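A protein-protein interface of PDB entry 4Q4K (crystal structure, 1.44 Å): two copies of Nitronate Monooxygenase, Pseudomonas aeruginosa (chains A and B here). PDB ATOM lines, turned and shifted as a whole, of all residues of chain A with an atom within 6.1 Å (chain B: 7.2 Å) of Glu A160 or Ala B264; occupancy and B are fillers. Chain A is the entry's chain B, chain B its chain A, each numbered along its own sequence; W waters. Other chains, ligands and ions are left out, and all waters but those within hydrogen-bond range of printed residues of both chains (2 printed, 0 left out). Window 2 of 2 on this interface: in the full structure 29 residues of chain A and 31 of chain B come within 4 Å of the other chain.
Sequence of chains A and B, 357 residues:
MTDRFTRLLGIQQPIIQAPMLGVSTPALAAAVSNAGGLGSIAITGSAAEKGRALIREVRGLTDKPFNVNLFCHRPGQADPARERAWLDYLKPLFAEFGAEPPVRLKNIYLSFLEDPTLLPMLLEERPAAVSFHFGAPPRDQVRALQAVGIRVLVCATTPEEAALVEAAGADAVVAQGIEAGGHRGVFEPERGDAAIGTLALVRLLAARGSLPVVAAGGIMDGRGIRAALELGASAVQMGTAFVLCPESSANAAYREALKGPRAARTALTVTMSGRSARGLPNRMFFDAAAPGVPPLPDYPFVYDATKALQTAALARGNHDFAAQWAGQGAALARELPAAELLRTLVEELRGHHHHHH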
ATOM      1  N   THR A 158     -25.580 -24.318  -9.920  1.00  0.00           N
ATOM      2  CA  THR A 158     -25.160 -23.074 -10.562  1.00  0.00           C
ATOM      3  C   THR A 158     -25.355 -21.902  -9.589  1.00  0.00           C
ATOM      4  O   THR A 158     -26.189 -22.072  -8.660  1.00  0.00           O
ATOM      5  CB  THR A 158     -25.994 -22.754 -11.817  1.00  0.00           C
ATOM      6  OG1 THR A 158     -27.348 -22.434 -11.419  1.00  0.00           O
ATOM      7  CG2 THR A 158     -26.012 -23.884 -12.800  1.00  0.00           C
ATOM      8  N   PRO A 159     -24.654 -20.759  -9.824  1.00  0.00           N
ATOM      9  CA  PRO A 159     -24.883 -19.493  -9.048  1.00  0.00           C
ATOM     10  C   PRO A 159     -26.332 -19.091  -9.143  1.00  0.00           C
ATOM     11  O   PRO A 159     -26.840 -18.604  -8.097  1.00  0.00           O
ATOM     12  CB  PRO A 159     -23.909 -18.462  -9.668  1.00  0.00           C
ATOM     13  CG  PRO A 159     -22.859 -19.333 -10.319  1.00  0.00           C
ATOM     14  CD  PRO A 159     -23.559 -20.573 -10.792  1.00  0.00           C
ATOM     15  N   GLU A 160     -27.023 -19.365 -10.244  1.00  0.00           N
ATOM     16  CA  GLU A 160     -28.394 -18.896 -10.434  1.00  0.00           C
ATOM     17  C   GLU A 160     -29.203 -19.700  -9.442  1.00  0.00           C
ATOM     18  O   GLU A 160     -29.883 -19.094  -8.583  1.00  0.00           O
ATOM     19  CB  GLU A 160     -28.891 -19.046 -11.871  1.00  0.00           C
ATOM     20  CG  GLU A 160     -28.250 -18.055 -12.870  1.00  0.00           C
ATOM     21  CD  GLU A 160     -26.729 -18.218 -13.091  1.00  0.00           C
ATOM     22  OE1 GLU A 160     -26.173 -19.359 -13.014  1.00  0.00           O
ATOM     23  OE2 GLU A 160     -26.047 -17.191 -13.348  1.00  0.00           O
ATOM     24  N   GLU A 161     -29.079 -21.054  -9.448  1.00  0.00           N
ATOM     25  CA  GLU A 161     -29.797 -21.878  -8.514  1.00  0.00           C
ATOM     26  C   GLU A 161     -29.382 -21.603  -7.075  1.00  0.00           C
ATOM     27  O   GLU A 161     -30.239 -21.705  -6.184  1.00  0.00           O
ATOM     28  CB  GLU A 161     -29.548 -23.388  -8.815  1.00  0.00           C
ATOM     29  CG  GLU A 161     -30.196 -23.857 -10.101  1.00  0.00           C
ATOM     30  CD  GLU A 161     -29.725 -25.230 -10.580  1.00  0.00           C
ATOM     31  OE1 GLU A 161     -28.776 -25.808  -9.939  1.00  0.00           O
ATOM     32  OE2 GLU A 161     -30.297 -25.745 -11.571  1.00  0.00           O
ATOM     33  N   ALA A 162     -28.133 -21.248  -6.794  1.00  0.00           N
ATOM     34  CA  ALA A 162     -27.700 -20.869  -5.428  1.00  0.00           C
ATOM     35  C   ALA A 162     -28.469 -19.593  -4.948  1.00  0.00           C
ATOM     36  O   ALA A 162     -28.734 -19.464  -3.745  1.00  0.00           O
ATOM     37  CB  ALA A 162     -26.219 -20.635  -5.284  1.00  0.00           C
ATOM     38  N   ALA A 163     -28.751 -18.684  -5.888  1.00  0.00           N
ATOM     39  CA  ALA A 163     -29.713 -17.547  -5.607  1.00  0.00           C
ATOM     40  C   ALA A 163     -31.058 -17.999  -5.106  1.00  0.00           C
ATOM     41  O   ALA A 163     -31.574 -17.396  -4.130  1.00  0.00           O
ATOM     42  CB  ALA A 163     -29.915 -16.679  -6.847  1.00  0.00           C
ATOM     43  N   LEU A 164     -31.679 -18.943  -5.811  1.00  0.00           N
ATOM     44  CA  LEU A 164     -32.988 -19.482  -5.492  1.00  0.00           C
ATOM     45  C   LEU A 164     -32.964 -20.199  -4.149  1.00  0.00           C
ATOM     46  O   LEU A 164     -34.004 -20.276  -3.471  1.00  0.00           O
ATOM     47  CB  LEU A 164     -33.564 -20.382  -6.605  1.00  0.00           C
ATOM     48  CG  LEU A 164     -33.862 -19.856  -8.022  1.00  0.00           C
ATOM     49  CD1 LEU A 164     -34.013 -21.003  -9.005  1.00  0.00           C
ATOM     50  CD2 LEU A 164     -35.171 -19.042  -8.031  1.00  0.00           C
ATOM     51  N   VAL A 165     -31.774 -20.666  -3.730  1.00  0.00           N
ATOM     52  CA  VAL A 165     -31.631 -21.324  -2.435  1.00  0.00           C
ATOM     53  C   VAL A 165     -31.579 -20.261  -1.332  1.00  0.00           C
ATOM     54  O   VAL A 165     -32.234 -20.412  -0.270  1.00  0.00           O
ATOM     55  CB  VAL A 165     -30.386 -22.254  -2.389  1.00  0.00           C
ATOM     56  CG1 VAL A 165     -30.170 -22.805  -0.971  1.00  0.00           C
ATOM     57  CG2 VAL A 165     -30.564 -23.406  -3.387  1.00  0.00           C
ATOM     58  N   ILE A 196     -21.243 -27.139 -14.493  1.00  0.00           N
ATOM     59  CA  ILE A 196     -20.097 -26.467 -13.879  1.00  0.00           C
ATOM     60  C   ILE A 196     -19.274 -27.372 -12.928  1.00  0.00           C
ATOM     61  O   ILE A 196     -19.850 -28.117 -12.157  1.00  0.00           O
ATOM     62  CB  ILE A 196     -20.531 -25.118 -13.086  1.00  0.00           C
ATOM     63  CG1 ILE A 196     -21.413 -24.226 -13.997  1.00  0.00           C
ATOM     64  CG2 ILE A 196     -19.353 -24.336 -12.509  1.00  0.00           C
ATOM     65  CD1 ILE A 196     -22.181 -23.125 -13.260  1.00  0.00           C
ATOM     66  N   LEU A 205     -19.747 -19.687  -5.594  1.00  0.00           N
ATOM     67  CA  LEU A 205     -20.725 -19.607  -4.484  1.00  0.00           C
ATOM     68  C   LEU A 205     -20.098 -19.083  -3.197  1.00  0.00           C
ATOM     69  O   LEU A 205     -20.778 -18.287  -2.484  1.00  0.00           O
ATOM     70  CB  LEU A 205     -21.489 -20.929  -4.264  1.00  0.00           C
ATOM     71  CG  LEU A 205     -22.308 -21.536  -5.380  1.00  0.00           C
ATOM     72  CD1 LEU A 205     -23.252 -22.610  -4.867  1.00  0.00           C
ATOM     73  CD2 LEU A 205     -23.006 -20.522  -6.270  1.00  0.00           C
ATOM     74  N   ARG A 208     -19.539 -15.299  -3.979  1.00  0.00           N
ATOM     75  CA  ARG A 208     -20.663 -14.425  -4.375  1.00  0.00           C
ATOM     76  C   ARG A 208     -21.956 -14.567  -3.587  1.00  0.00           C
ATOM     77  O   ARG A 208     -22.796 -13.651  -3.567  1.00  0.00           O
ATOM     78  CB  ARG A 208     -20.877 -14.475  -5.871  1.00  0.00           C
ATOM     79  CG  ARG A 208     -19.679 -13.861  -6.584  1.00  0.00           C
ATOM     80  CD  ARG A 208     -19.487 -14.500  -7.934  1.00  0.00           C
ATOM     81  NE  ARG A 208     -20.523 -14.088  -8.878  1.00  0.00           N
ATOM     82  CZ  ARG A 208     -20.501 -12.956  -9.583  1.00  0.00           C
ATOM     83  NH1 ARG A 208     -19.494 -12.086  -9.492  1.00  0.00           N
ATOM     84  NH2 ARG A 208     -21.489 -12.723 -10.420  1.00  0.00           N
ATOM     85  N   ALA B 257     -17.784  -7.961 -22.971  1.00  0.00           N
ATOM     86  CA  ALA B 257     -18.500  -9.227 -22.826  1.00  0.00           C
ATOM     87  C   ALA B 257     -18.060  -9.946 -21.539  1.00  0.00           C
ATOM     88  O   ALA B 257     -18.869 -10.331 -20.718  1.00  0.00           O
ATOM     89  CB  ALA B 257     -18.207 -10.111 -24.036  1.00  0.00           C
ATOM     90  N   LEU B 258     -16.763  -9.963 -21.320  1.00  0.00           N
ATOM     91  CA  LEU B 258     -16.214 -10.707 -20.183  1.00  0.00           C
ATOM     92  C   LEU B 258     -16.401  -9.980 -18.840  1.00  0.00           C
ATOM     93  O   LEU B 258     -16.626 -10.601 -17.782  1.00  0.00           O
ATOM     94  CB  LEU B 258     -14.757 -11.032 -20.449  1.00  0.00           C
ATOM     95  CG  LEU B 258     -13.957 -11.837 -19.419  1.00  0.00           C
ATOM     96  CD1 LEU B 258     -14.696 -13.150 -19.115  1.00  0.00           C
ATOM     97  CD2 LEU B 258     -12.577 -12.099 -19.954  1.00  0.00           C
ATOM     98  N   GLY B 260     -18.966  -8.093 -18.162  1.00  0.00           N
ATOM     99  CA  GLY B 260     -20.403  -7.951 -18.006  1.00  0.00           C
ATOM    100  C   GLY B 260     -21.159  -9.173 -17.511  1.00  0.00           C
ATOM    101  O   GLY B 260     -20.528 -10.148 -17.074  1.00  0.00           O
ATOM    102  N   PRO B 261     -22.508  -9.172 -17.615  1.00  0.00           N
ATOM    103  CA  PRO B 261     -23.324 -10.246 -17.041  1.00  0.00           C
ATOM    104  C   PRO B 261     -23.217 -11.587 -17.794  1.00  0.00           C
ATOM    105  O   PRO B 261     -23.586 -12.632 -17.248  1.00  0.00           O
ATOM    106  CB  PRO B 261     -24.767  -9.711 -17.168  1.00  0.00           C
ATOM    107  CG  PRO B 261     -24.622  -8.265 -17.493  1.00  0.00           C
ATOM    108  CD  PRO B 261     -23.366  -8.161 -18.281  1.00  0.00           C
ATOM    109  N   ARG B 262     -22.782 -11.544 -19.055  1.00  0.00           N
ATOM    110  CA  ARG B 262     -22.699 -12.798 -19.839  1.00  0.00           C
ATOM    111  C   ARG B 262     -21.630 -13.728 -19.224  1.00  0.00           C
ATOM    112  O   ARG B 262     -21.727 -14.950 -19.398  1.00  0.00           O
ATOM    113  CB  ARG B 262     -22.366 -12.515 -21.315  1.00  0.00           C
ATOM    114  CG  ARG B 262     -23.361 -11.684 -22.107  1.00  0.00           C
ATOM    115  CD  ARG B 262     -22.717 -11.150 -23.385  1.00  0.00           C
ATOM    116  NE  ARG B 262     -22.349 -12.315 -24.243  1.00  0.00           N
ATOM    117  CZ  ARG B 262     -21.516 -12.238 -25.277  1.00  0.00           C
ATOM    118  NH1 ARG B 262     -20.961 -11.050 -25.610  1.00  0.00           N
ATOM    119  NH2 ARG B 262     -21.226 -13.355 -26.003  1.00  0.00           N
ATOM    120  N   ALA B 263     -20.697 -13.166 -18.451  1.00  0.00           N
ATOM    121  CA  ALA B 263     -19.595 -13.921 -17.858  1.00  0.00           C
ATOM    122  C   ALA B 263     -20.136 -14.964 -16.869  1.00  0.00           C
ATOM    123  O   ALA B 263     -19.450 -15.927 -16.519  1.00  0.00           O
ATOM    124  CB  ALA B 263     -18.591 -12.998 -17.196  1.00  0.00           C
ATOM    125  N   ALA B 264     -21.365 -14.767 -16.412  1.00  0.00           N
ATOM    126  CA  ALA B 264     -21.956 -15.698 -15.461  1.00  0.00           C
ATOM    127  C   ALA B 264     -22.293 -17.049 -16.093  1.00  0.00           C
ATOM    128  O   ALA B 264     -22.512 -18.018 -15.374  1.00  0.00           O
ATOM    129  CB  ALA B 264     -23.207 -15.095 -14.856  1.00  0.00           C
ATOM    130  N   ARG B 265     -22.323 -17.142 -17.413  1.00  0.00           N
ATOM    131  CA  ARG B 265     -22.653 -18.432 -18.025  1.00  0.00           C
ATOM    132  C   ARG B 265     -21.879 -18.658 -19.297  1.00  0.00           C
ATOM    133  O   ARG B 265     -21.980 -17.932 -20.254  1.00  0.00           O
ATOM    134  CB  ARG B 265     -24.116 -18.573 -18.303  1.00  0.00           C
ATOM    135  CG  ARG B 265     -24.529 -19.902 -18.926  1.00  0.00           C
ATOM    136  CD  ARG B 265     -24.287 -21.023 -17.947  1.00  0.00           C
ATOM    137  NE  ARG B 265     -25.029 -20.843 -16.680  1.00  0.00           N
ATOM    138  CZ  ARG B 265     -26.303 -21.195 -16.474  1.00  0.00           C
ATOM    139  NH1 ARG B 265     -27.009 -21.794 -17.421  1.00  0.00           N
ATOM    140  NH2 ARG B 265     -26.867 -20.997 -15.269  1.00  0.00           N
ATOM    141  N   THR B 266     -21.121 -19.733 -19.290  1.00  0.00           N
ATOM    142  CA  THR B 266     -20.346 -20.155 -20.461  1.00  0.00           C
ATOM    143  C   THR B 266     -20.991 -21.402 -20.989  1.00  0.00           C
ATOM    144  O   THR B 266     -21.816 -22.064 -20.337  1.00  0.00           O
ATOM    145  CB  THR B 266     -18.846 -20.383 -20.158  1.00  0.00           C
ATOM    146  OG1 THR B 266     -18.724 -21.537 -19.258  1.00  0.00           O
ATOM    147  CG2 THR B 266     -18.172 -19.187 -19.490  1.00  0.00           C
ATOM    148  N   LEU B 280     -18.465 -17.529 -24.227  1.00  0.00           N
ATOM    149  CA  LEU B 280     -19.716 -16.805 -23.852  1.00  0.00           C
ATOM    150  C   LEU B 280     -20.638 -17.016 -25.026  1.00  0.00           C
ATOM    151  O   LEU B 280     -20.277 -16.540 -26.151  1.00  0.00           O
ATOM    152  CB  LEU B 280     -19.344 -15.316 -23.665  1.00  0.00           C
ATOM    153  CG  LEU B 280     -18.266 -15.023 -22.650  1.00  0.00           C
ATOM    154  CD1 LEU B 280     -17.934 -13.525 -22.586  1.00  0.00           C
ATOM    155  CD2 LEU B 280     -18.609 -15.572 -21.264  1.00  0.00           C
ATOM    156  N   GLN B 328     -15.157 -21.306 -16.797  1.00  0.00           N
ATOM    157  CA  GLN B 328     -16.307 -21.253 -15.900  1.00  0.00           C
ATOM    158  C   GLN B 328     -16.104 -20.322 -14.670  1.00  0.00           C
ATOM    159  O   GLN B 328     -17.115 -20.088 -13.983  1.00  0.00           O
ATOM    160  CB  GLN B 328     -16.701 -22.680 -15.430  1.00  0.00           C
ATOM    161  CG  GLN B 328     -17.312 -23.436 -16.600  1.00  0.00           C
ATOM    162  CD  GLN B 328     -17.719 -24.895 -16.239  1.00  0.00           C
ATOM    163  OE1 GLN B 328     -17.144 -25.479 -15.315  1.00  0.00           O
ATOM    164  NE2 GLN B 328     -18.685 -25.450 -16.924  1.00  0.00           N
ATOM    165  N   ALA B 330     -15.262 -17.202 -15.112  1.00  0.00           N
ATOM    166  CA  ALA B 330     -15.157 -15.879 -15.811  1.00  0.00           C
ATOM    167  C   ALA B 330     -15.708 -14.745 -14.914  1.00  0.00           C
ATOM    168  O   ALA B 330     -15.099 -13.626 -14.982  1.00  0.00           O
ATOM    169  CB  ALA B 330     -15.878 -15.915 -17.125  1.00  0.00           C
ATOM    170  N   ALA B 331     -16.734 -15.012 -14.133  1.00  0.00           N
ATOM    171  CA  ALA B 331     -17.303 -13.917 -13.284  1.00  0.00           C
ATOM    172  C   ALA B 331     -16.330 -13.378 -12.259  1.00  0.00           C
ATOM    173  O   ALA B 331     -16.578 -12.257 -11.703  1.00  0.00           O
ATOM    174  CB  ALA B 331     -18.548 -14.424 -12.604  1.00  0.00           C
HETATM  175  O   HOH W   1     -24.160 -19.983 -14.566  1.00  0.00           O
HETATM  176  O   HOH W   2     -28.952 -22.441 -13.464  1.00  0.00           O
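OG1 of Thr A158 sits at hydrogen-bond distance from N of Glu A161 (3.0 Å).
The backbone NH (N) of Glu A160 lies close to the side-chain hydroxyl (OG1) of Thr A158 (3.3 Å).
No position is printed for both chains.
Of the 5 pairs that touch across the chains among the printed residues, none has its exchanged pair printed and touching as well.
NH2 of Arg B265 touches CG2 of Thr A158 (3.9 Å).
Ala B264 touches Glu A160 (CB to OE2, 3.8 Å).
OE1 of Gln B328 touches CA of Ile A196, 3.4 Å away.
Arg A208 touches Ala B331.
Water W1 lies within hydrogen-bond range of NE of Arg B265 (2.4 Å), OE1 of Glu A160 (2.6 Å) and O of Ala B264 (2.7 Å).
Water W2 bridges the side-chain hydroxyl of Thr A158 (2.6 Å) and the guanidinium group of Arg B265 (3.1 Å).
Of the 13 printed residues of chain B, 4 touch a printed residue of chain A.
Among the printed residues, 5 pairs touch across the chains.
Glu A160 touches just these residues of chain B: Ala B264 and Arg B265.
Of the printed residues of chain B, Ile A196 touches Gln B328.
Of the printed residues of chain A, Arg B265 touches Thr A158 (3.9 Å) and Glu A160 (2.9 Å).
Of the printed residues of chain B, Thr A158 touches Arg B265 (3.9 Å).
Ala B330 touches none of the printed residues of chain A.
Ala A163 touches none of the printed residues of chain B.
The nearest residue of chain B that does not touch Glu A160 is Pro B261 (6.5 Å).
The nearest printed residue of chain B that does not touch Thr A158 is Ala B264 (6.9 Å).
The guanidinium group (NH2) of Arg B265 lies within salt-bridge range of the side-chain carboxylate (OE1) of Glu A160 (2.9 Å).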
